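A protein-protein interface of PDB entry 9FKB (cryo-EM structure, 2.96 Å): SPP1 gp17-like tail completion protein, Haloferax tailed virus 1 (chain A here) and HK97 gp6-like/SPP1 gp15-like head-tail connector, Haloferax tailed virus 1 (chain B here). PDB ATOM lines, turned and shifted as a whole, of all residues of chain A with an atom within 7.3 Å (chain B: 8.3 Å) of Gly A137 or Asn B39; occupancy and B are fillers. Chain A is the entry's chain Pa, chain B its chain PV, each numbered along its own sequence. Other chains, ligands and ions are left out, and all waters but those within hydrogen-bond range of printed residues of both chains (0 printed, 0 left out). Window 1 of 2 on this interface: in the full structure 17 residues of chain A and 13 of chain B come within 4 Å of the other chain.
The backbone carbonyl oxygen of Phe A87 is in hydrogen-bond range of the side-chain amide nitrogen of Asn B39 (3.0 Å). OG1 of Thr A136 sits at hydrogen-bond distance from N of Asn B39, at 3.4 Å. The side-chain carboxylate of Glu B90 is in hydrogen-bond range of the backbone NH of Thr A136, at 2.9 Å.
The side-chain hydroxyl (OG1) of Thr B40 lies within hydrogen-bond range of the side-chain carboxylate (OE2) of Glu B90 (2.6 Å). The backbone carbonyl oxygen (O) of Ser A86 is in hydrogen-bond range of the backbone NH (N) of Tyr A139, 2.8 Å away.
CZ of Phe A87 touches CA of Thr B35 (3.9 Å). Val B38 touches Phe A87 (CG2 to CB, 3.7 Å). CD of Arg A134 touches O of Glu B90 (3.4 Å). CA of Thr A135 touches OE1 of Glu B90, 3.5 Å away. Thr B35 touches Thr A136 (OG1 to CG2, 3.4 Å). Trp B37 touches Thr A136. Thr A136 touches Val B38 (OG1 to N, 3.7 Å). Gly A137 touches Asn B39 (O to ND2, 3.9 Å). CE2 of Tyr A139 touches ND2 of Asn B39, 3.8 Å away.
Ala A133 touches none of the printed residues of chain B. Thr A136 touches just these residues of chain B: Thr B35, Trp B37, Val B38, Asn B39 and Glu B90. Of chain B, only Asn B39 comes within 4 Å of Gly A137. Printed residues of chain B within 4 Å of Tyr A139: Asn B39. Printed residues of chain A within 4 Å of Val B38: Phe A87 (3.7 Å) and Thr A136 (3.7 Å). Of chain A, only Phe A87 (3.0 Å), Thr A136 (3.4 Å), Gly A137 (3.9 Å) and Tyr A139 (3.8 Å) come within 4 Å of Asn B39. The nearest printed residue of chain A that does not touch Asn B39 is Asp A88 (5.1 Å).
Hydrophobic or aromatic side chains of chain B that line the printed part of chain A: Val B38. Along chain A the printed residues that touch a printed residue of chain B span positions 87 to 139. Among the printed residues, 12 pairs touch across the chains. Among the printed residues, no Asp or Glu carboxylate lies within 4 Å of a Lys or Arg side-chain nitrogen of the other chain.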
ATOM      1  N   SER A  86     -26.200 -13.466  30.106  1.00  0.00           N
ATOM      2  CA  SER A  86     -27.097 -12.674  29.266  1.00  0.00           C
ATOM      3  C   SER A  86     -27.171 -11.229  29.768  1.00  0.00           C
ATOM      4  O   SER A  86     -26.834 -10.944  30.909  1.00  0.00           O
ATOM      5  CB  SER A  86     -28.489 -13.273  29.197  1.00  0.00           C
ATOM      6  OG  SER A  86     -29.359 -12.459  28.422  1.00  0.00           O
ATOM      7  N   PHE A  87     -27.640 -10.302  28.919  1.00  0.00           N
ATOM      8  CA  PHE A  87     -27.965  -8.947  29.353  1.00  0.00           C
ATOM      9  C   PHE A  87     -29.276  -8.890  30.143  1.00  0.00           C
ATOM     10  O   PHE A  87     -29.533  -7.906  30.835  1.00  0.00           O
ATOM     11  CB  PHE A  87     -28.044  -8.034  28.135  1.00  0.00           C
ATOM     12  CG  PHE A  87     -26.721  -7.898  27.419  1.00  0.00           C
ATOM     13  CD1 PHE A  87     -25.659  -7.206  28.009  1.00  0.00           C
ATOM     14  CD2 PHE A  87     -26.534  -8.503  26.178  1.00  0.00           C
ATOM     15  CE1 PHE A  87     -24.442  -7.101  27.348  1.00  0.00           C
ATOM     16  CE2 PHE A  87     -25.325  -8.377  25.503  1.00  0.00           C
ATOM     17  CZ  PHE A  87     -24.283  -7.690  26.107  1.00  0.00           C
ATOM     18  N   ASP A  88     -30.114  -9.928  30.043  1.00  0.00           N
ATOM     19  CA  ASP A  88     -31.431  -9.957  30.664  1.00  0.00           C
ATOM     20  C   ASP A  88     -31.383 -10.688  32.008  1.00  0.00           C
ATOM     21  O   ASP A  88     -31.197 -11.900  32.065  1.00  0.00           O
ATOM     22  CB  ASP A  88     -32.435 -10.517  29.654  1.00  0.00           C
ATOM     23  CG  ASP A  88     -33.874 -10.635  30.144  1.00  0.00           C
ATOM     24  OD1 ASP A  88     -34.114 -10.497  31.358  1.00  0.00           O
ATOM     25  OD2 ASP A  88     -34.766 -10.851  29.289  1.00  0.00           O
ATOM     26  N   GLU A  89     -31.618  -9.940  33.094  1.00  0.00           N
ATOM     27  CA  GLU A  89     -31.608 -10.465  34.457  1.00  0.00           C
ATOM     28  C   GLU A  89     -32.674 -11.540  34.700  1.00  0.00           C
ATOM     29  O   GLU A  89     -32.468 -12.422  35.534  1.00  0.00           O
ATOM     30  CB  GLU A  89     -31.738  -9.329  35.473  1.00  0.00           C
ATOM     31  CG  GLU A  89     -32.951  -8.439  35.252  1.00  0.00           C
ATOM     32  CD  GLU A  89     -32.970  -7.168  36.087  1.00  0.00           C
ATOM     33  OE1 GLU A  89     -32.839  -7.275  37.324  1.00  0.00           O
ATOM     34  OE2 GLU A  89     -33.120  -6.068  35.501  1.00  0.00           O
ATOM     35  N   THR A 131     -22.740  -7.047  38.438  1.00  0.00           N
ATOM     36  CA  THR A 131     -22.889  -6.254  37.224  1.00  0.00           C
ATOM     37  C   THR A 131     -23.125  -4.793  37.601  1.00  0.00           C
ATOM     38  O   THR A 131     -24.099  -4.486  38.277  1.00  0.00           O
ATOM     39  CB  THR A 131     -24.049  -6.774  36.367  1.00  0.00           C
ATOM     40  OG1 THR A 131     -23.857  -8.167  36.126  1.00  0.00           O
ATOM     41  CG2 THR A 131     -24.169  -6.080  35.030  1.00  0.00           C
ATOM     42  N   PRO A 132     -22.260  -3.834  37.177  1.00  0.00           N
ATOM     43  CA  PRO A 132     -22.532  -2.415  37.419  1.00  0.00           C
ATOM     44  C   PRO A 132     -23.809  -1.990  36.687  1.00  0.00           C
ATOM     45  O   PRO A 132     -24.022  -2.348  35.527  1.00  0.00           O
ATOM     46  CB  PRO A 132     -21.299  -1.689  36.858  1.00  0.00           C
ATOM     47  CG  PRO A 132     -20.229  -2.764  36.706  1.00  0.00           C
ATOM     48  CD  PRO A 132     -20.989  -4.051  36.463  1.00  0.00           C
ATOM     49  N   ALA A 133     -24.669  -1.234  37.380  1.00  0.00           N
ATOM     50  CA  ALA A 133     -25.953  -0.803  36.832  1.00  0.00           C
ATOM     51  C   ALA A 133     -25.832   0.317  35.782  1.00  0.00           C
ATOM     52  O   ALA A 133     -26.733   0.464  34.943  1.00  0.00           O
ATOM     53  CB  ALA A 133     -26.884  -0.412  37.953  1.00  0.00           C
ATOM     54  N   ARG A 134     -24.744   1.116  35.834  1.00  0.00           N
ATOM     55  CA  ARG A 134     -24.596   2.316  35.014  1.00  0.00           C
ATOM     56  C   ARG A 134     -24.442   1.960  33.534  1.00  0.00           C
ATOM     57  O   ARG A 134     -25.063   2.594  32.673  1.00  0.00           O
ATOM     58  CB  ARG A 134     -23.471   3.225  35.527  1.00  0.00           C
ATOM     59  CG  ARG A 134     -23.469   4.595  34.869  1.00  0.00           C
ATOM     60  CD  ARG A 134     -22.212   5.443  34.966  1.00  0.00           C
ATOM     61  NE  ARG A 134     -22.004   5.778  36.369  1.00  0.00           N
ATOM     62  CZ  ARG A 134     -22.797   6.567  37.090  1.00  0.00           C
ATOM     63  NH1 ARG A 134     -22.513   6.806  38.363  1.00  0.00           N
ATOM     64  NH2 ARG A 134     -23.834   7.176  36.538  1.00  0.00           N
ATOM     65  N   THR A 135     -23.589   0.973  33.246  1.00  0.00           N
ATOM     66  CA  THR A 135     -23.396   0.488  31.888  1.00  0.00           C
ATOM     67  C   THR A 135     -24.404  -0.615  31.555  1.00  0.00           C
ATOM     68  O   THR A 135     -24.946  -1.268  32.440  1.00  0.00           O
ATOM     69  CB  THR A 135     -21.966  -0.033  31.675  1.00  0.00           C
ATOM     70  OG1 THR A 135     -21.767  -1.274  32.353  1.00  0.00           O
ATOM     71  CG2 THR A 135     -20.898   0.940  32.127  1.00  0.00           C
ATOM     72  N   THR A 136     -24.623  -0.863  30.258  1.00  0.00           N
ATOM     73  CA  THR A 136     -25.064  -2.187  29.851  1.00  0.00           C
ATOM     74  C   THR A 136     -23.940  -3.184  30.153  1.00  0.00           C
ATOM     75  O   THR A 136     -22.767  -2.812  30.152  1.00  0.00           O
ATOM     76  CB  THR A 136     -25.515  -2.179  28.387  1.00  0.00           C
ATOM     77  OG1 THR A 136     -26.364  -3.302  28.145  1.00  0.00           O
ATOM     78  CG2 THR A 136     -24.359  -2.180  27.412  1.00  0.00           C
ATOM     79  N   GLY A 137     -24.290  -4.447  30.431  1.00  0.00           N
ATOM     80  CA  GLY A 137     -23.306  -5.462  30.787  1.00  0.00           C
ATOM     81  C   GLY A 137     -23.979  -6.795  31.102  1.00  0.00           C
ATOM     82  O   GLY A 137     -25.164  -6.832  31.431  1.00  0.00           O
ATOM     83  N   HIS A 138     -23.224  -7.892  30.974  1.00  0.00           N
ATOM     84  CA  HIS A 138     -23.775  -9.210  31.253  1.00  0.00           C
ATOM     85  C   HIS A 138     -24.089  -9.399  32.733  1.00  0.00           C
ATOM     86  O   HIS A 138     -23.278  -9.086  33.590  1.00  0.00           O
ATOM     87  CB  HIS A 138     -22.818 -10.302  30.780  1.00  0.00           C
ATOM     88  CG  HIS A 138     -22.540 -10.228  29.316  1.00  0.00           C
ATOM     89  ND1 HIS A 138     -21.332  -9.780  28.782  1.00  0.00           N
ATOM     90  CD2 HIS A 138     -23.338 -10.518  28.272  1.00  0.00           C
ATOM     91  CE1 HIS A 138     -21.405  -9.824  27.470  1.00  0.00           C
ATOM     92  NE2 HIS A 138     -22.628 -10.274  27.135  1.00  0.00           N
ATOM     93  N   TYR A 139     -25.275  -9.950  33.001  1.00  0.00           N
ATOM     94  CA  TYR A 139     -25.549 -10.652  34.241  1.00  0.00           C
ATOM     95  C   TYR A 139     -25.031 -12.083  34.140  1.00  0.00           C
ATOM     96  O   TYR A 139     -25.050 -12.668  33.064  1.00  0.00           O
ATOM     97  CB  TYR A 139     -27.050 -10.641  34.496  1.00  0.00           C
ATOM     98  CG  TYR A 139     -27.573  -9.249  34.722  1.00  0.00           C
ATOM     99  CD1 TYR A 139     -27.161  -8.511  35.831  1.00  0.00           C
ATOM    100  CD2 TYR A 139     -28.455  -8.661  33.826  1.00  0.00           C
ATOM    101  CE1 TYR A 139     -27.608  -7.208  36.030  1.00  0.00           C
ATOM    102  CE2 TYR A 139     -28.911  -7.362  34.024  1.00  0.00           C
ATOM    103  CZ  TYR A 139     -28.490  -6.633  35.129  1.00  0.00           C
ATOM    104  OH  TYR A 139     -28.936  -5.354  35.340  1.00  0.00           O
ATOM    105  N   ILE A 140     -24.580 -12.637  35.275  1.00  0.00           N
ATOM    106  CA  ILE A 140     -24.094 -14.010  35.336  1.00  0.00           C
ATOM    107  C   ILE A 140     -24.784 -14.748  36.484  1.00  0.00           C
ATOM    108  O   ILE A 140     -24.953 -14.212  37.578  1.00  0.00           O
ATOM    109  CB  ILE A 140     -22.545 -14.078  35.426  1.00  0.00           C
ATOM    110  CG1 ILE A 140     -21.880 -13.296  34.287  1.00  0.00           C
ATOM    111  CG2 ILE A 140     -22.056 -15.528  35.437  1.00  0.00           C
ATOM    112  CD1 ILE A 140     -20.378 -13.193  34.366  1.00  0.00           C
ATOM    113  N   GLU B  30     -28.057   1.269  17.169  1.00  0.00           N
ATOM    114  CA  GLU B  30     -27.813   0.123  18.038  1.00  0.00           C
ATOM    115  C   GLU B  30     -26.890  -0.924  17.405  1.00  0.00           C
ATOM    116  O   GLU B  30     -26.354  -1.769  18.108  1.00  0.00           O
ATOM    117  CB  GLU B  30     -29.136  -0.537  18.415  1.00  0.00           C
ATOM    118  CG  GLU B  30     -29.953   0.217  19.451  1.00  0.00           C
ATOM    119  CD  GLU B  30     -31.267  -0.464  19.808  1.00  0.00           C
ATOM    120  OE1 GLU B  30     -31.689  -1.379  19.060  1.00  0.00           O
ATOM    121  OE2 GLU B  30     -31.871  -0.099  20.846  1.00  0.00           O
ATOM    122  N   THR B  35     -23.022  -4.883  22.225  1.00  0.00           N
ATOM    123  CA  THR B  35     -23.879  -4.842  23.405  1.00  0.00           C
ATOM    124  C   THR B  35     -25.210  -4.127  23.141  1.00  0.00           C
ATOM    125  O   THR B  35     -26.120  -4.214  23.966  1.00  0.00           O
ATOM    126  CB  THR B  35     -23.141  -4.187  24.582  1.00  0.00           C
ATOM    127  OG1 THR B  35     -23.017  -2.780  24.365  1.00  0.00           O
ATOM    128  CG2 THR B  35     -21.769  -4.775  24.836  1.00  0.00           C
ATOM    129  N   GLY B  36     -25.320  -3.380  22.032  1.00  0.00           N
ATOM    130  CA  GLY B  36     -26.543  -2.699  21.615  1.00  0.00           C
ATOM    131  C   GLY B  36     -27.077  -1.638  22.590  1.00  0.00           C
ATOM    132  O   GLY B  36     -28.148  -1.081  22.358  1.00  0.00           O
ATOM    133  N   TRP B  37     -26.366  -1.374  23.700  1.00  0.00           N
ATOM    134  CA  TRP B  37     -26.859  -0.589  24.830  1.00  0.00           C
ATOM    135  C   TRP B  37     -28.256  -1.037  25.297  1.00  0.00           C
ATOM    136  O   TRP B  37     -29.063  -0.209  25.723  1.00  0.00           O
ATOM    137  CB  TRP B  37     -26.782   0.909  24.500  1.00  0.00           C
ATOM    138  CG  TRP B  37     -25.413   1.346  24.074  1.00  0.00           C
ATOM    139  CD1 TRP B  37     -24.368   1.643  24.894  1.00  0.00           C
ATOM    140  CD2 TRP B  37     -24.918   1.501  22.720  1.00  0.00           C
ATOM    141  NE1 TRP B  37     -23.276   2.002  24.147  1.00  0.00           N
ATOM    142  CE2 TRP B  37     -23.568   1.917  22.806  1.00  0.00           C
ATOM    143  CE3 TRP B  37     -25.462   1.323  21.435  1.00  0.00           C
ATOM    144  CZ2 TRP B  37     -22.791   2.183  21.660  1.00  0.00           C
ATOM    145  CZ3 TRP B  37     -24.696   1.568  20.303  1.00  0.00           C
ATOM    146  CH2 TRP B  37     -23.367   2.000  20.412  1.00  0.00           C
ATOM    147  N   VAL B  38     -28.513  -2.356  25.297  1.00  0.00           N
ATOM    148  CA  VAL B  38     -29.859  -2.906  25.477  1.00  0.00           C
ATOM    149  C   VAL B  38     -30.465  -2.619  26.854  1.00  0.00           C
ATOM    150  O   VAL B  38     -31.688  -2.506  26.965  1.00  0.00           O
ATOM    151  CB  VAL B  38     -29.928  -4.402  25.141  1.00  0.00           C
ATOM    152  CG1 VAL B  38     -29.685  -4.633  23.664  1.00  0.00           C
ATOM    153  CG2 VAL B  38     -28.952  -5.224  25.969  1.00  0.00           C
ATOM    154  N   ASN B  39     -29.627  -2.433  27.887  1.00  0.00           N
ATOM    155  CA  ASN B  39     -30.101  -2.117  29.233  1.00  0.00           C
ATOM    156  C   ASN B  39     -30.265  -0.613  29.502  1.00  0.00           C
ATOM    157  O   ASN B  39     -30.640  -0.223  30.610  1.00  0.00           O
ATOM    158  CB  ASN B  39     -29.287  -2.855  30.297  1.00  0.00           C
ATOM    159  CG  ASN B  39     -29.476  -4.360  30.260  1.00  0.00           C
ATOM    160  OD1 ASN B  39     -30.363  -4.869  29.574  1.00  0.00           O
ATOM    161  ND2 ASN B  39     -28.646  -5.081  30.997  1.00  0.00           N
ATOM    162  N   THR B  40     -30.025   0.232  28.485  1.00  0.00           N
ATOM    163  CA  THR B  40     -30.392   1.649  28.491  1.00  0.00           C
ATOM    164  C   THR B  40     -31.635   1.826  27.619  1.00  0.00           C
ATOM    165  O   THR B  40     -31.648   1.368  26.479  1.00  0.00           O
ATOM    166  CB  THR B  40     -29.188   2.511  28.073  1.00  0.00           C
ATOM    167  OG1 THR B  40     -28.357   2.701  29.214  1.00  0.00           O
ATOM    168  CG2 THR B  40     -29.534   3.899  27.578  1.00  0.00           C
ATOM    169  N   SER B  41     -32.676   2.491  28.148  1.00  0.00           N
ATOM    170  CA  SER B  41     -34.022   2.481  27.567  1.00  0.00           C
ATOM    171  C   SER B  41     -34.145   3.245  26.235  1.00  0.00           C
ATOM    172  O   SER B  41     -33.290   4.058  25.883  1.00  0.00           O
ATOM    173  CB  SER B  41     -35.049   2.946  28.575  1.00  0.00           C
ATOM    174  OG  SER B  41     -35.022   4.365  28.739  1.00  0.00           O
ATOM    175  N   ARG B  42     -35.251   3.013  25.501  1.00  0.00           N
ATOM    176  CA  ARG B  42     -35.522   3.644  24.213  1.00  0.00           C
ATOM    177  C   ARG B  42     -35.373   5.167  24.267  1.00  0.00           C
ATOM    178  O   ARG B  42     -34.729   5.747  23.400  1.00  0.00           O
ATOM    179  CB  ARG B  42     -36.917   3.277  23.707  1.00  0.00           C
ATOM    180  CG  ARG B  42     -37.199   3.825  22.319  1.00  0.00           C
ATOM    181  CD  ARG B  42     -38.666   3.933  21.950  1.00  0.00           C
ATOM    182  NE  ARG B  42     -38.797   4.513  20.628  1.00  0.00           N
ATOM    183  CZ  ARG B  42     -39.012   5.796  20.337  1.00  0.00           C
ATOM    184  NH1 ARG B  42     -39.080   6.135  19.068  1.00  0.00           N
ATOM    185  NH2 ARG B  42     -39.169   6.728  21.264  1.00  0.00           N
ATOM    186  N   ARG B  44     -33.672   7.175  26.033  1.00  0.00           N
ATOM    187  CA  ARG B  44     -32.285   7.615  26.136  1.00  0.00           C
ATOM    188  C   ARG B  44     -31.571   7.525  24.786  1.00  0.00           C
ATOM    189  O   ARG B  44     -30.828   8.427  24.416  1.00  0.00           O
ATOM    190  CB  ARG B  44     -31.599   6.826  27.249  1.00  0.00           C
ATOM    191  CG  ARG B  44     -32.306   7.041  28.573  1.00  0.00           C
ATOM    192  CD  ARG B  44     -31.707   6.336  29.770  1.00  0.00           C
ATOM    193  NE  ARG B  44     -32.129   6.928  31.030  1.00  0.00           N
ATOM    194  CZ  ARG B  44     -33.289   6.734  31.662  1.00  0.00           C
ATOM    195  NH1 ARG B  44     -33.499   7.348  32.813  1.00  0.00           N
ATOM    196  NH2 ARG B  44     -34.228   5.944  31.174  1.00  0.00           N
ATOM    197  N   LYS B  45     -31.850   6.472  24.016  1.00  0.00           N
ATOM    198  CA  LYS B  45     -31.325   6.291  22.668  1.00  0.00           C
ATOM    199  C   LYS B  45     -31.924   7.297  21.684  1.00  0.00           C
ATOM    200  O   LYS B  45     -31.187   7.937  20.934  1.00  0.00           O
ATOM    201  CB  LYS B  45     -31.466   4.823  22.262  1.00  0.00           C
ATOM    202  CG  LYS B  45     -30.533   3.932  23.065  1.00  0.00           C
ATOM    203  CD  LYS B  45     -30.698   2.441  22.845  1.00  0.00           C
ATOM    204  CE  LYS B  45     -31.959   1.887  23.479  1.00  0.00           C
ATOM    205  NZ  LYS B  45     -31.946   0.405  23.514  1.00  0.00           N
ATOM    206  N   GLU B  90     -24.045   6.456  29.466  1.00  0.00           N
ATOM    207  CA  GLU B  90     -23.623   5.313  30.279  1.00  0.00           C
ATOM    208  C   GLU B  90     -22.353   5.564  31.116  1.00  0.00           C
ATOM    209  O   GLU B  90     -21.787   4.615  31.661  1.00  0.00           O
ATOM    210  CB  GLU B  90     -23.438   4.080  29.394  1.00  0.00           C
ATOM    211  CG  GLU B  90     -24.729   3.611  28.745  1.00  0.00           C
ATOM    212  CD  GLU B  90     -24.891   2.100  28.663  1.00  0.00           C
ATOM    213  OE1 GLU B  90     -23.861   1.390  28.587  1.00  0.00           O
ATOM    214  OE2 GLU B  90     -26.051   1.623  28.699  1.00  0.00           O
ATOM    215  N   GLU B  97     -12.768  -3.794  33.511  1.00  0.00           N
ATOM    216  CA  GLU B  97     -13.931  -4.516  34.018  1.00  0.00           C
ATOM    217  C   GLU B  97     -13.490  -5.787  34.753  1.00  0.00           C
ATOM    218  O   GLU B  97     -12.505  -6.414  34.383  1.00  0.00           O
ATOM    219  CB  GLU B  97     -14.880  -4.916  32.892  1.00  0.00           C
ATOM    220  CG  GLU B  97     -15.598  -3.738  32.234  1.00  0.00           C
ATOM    221  CD  GLU B  97     -16.552  -4.188  31.121  1.00  0.00           C
ATOM    222  OE1 GLU B  97     -16.066  -4.740  30.107  1.00  0.00           O
ATOM    223  OE2 GLU B  97     -17.797  -4.005  31.267  1.00  0.00           O
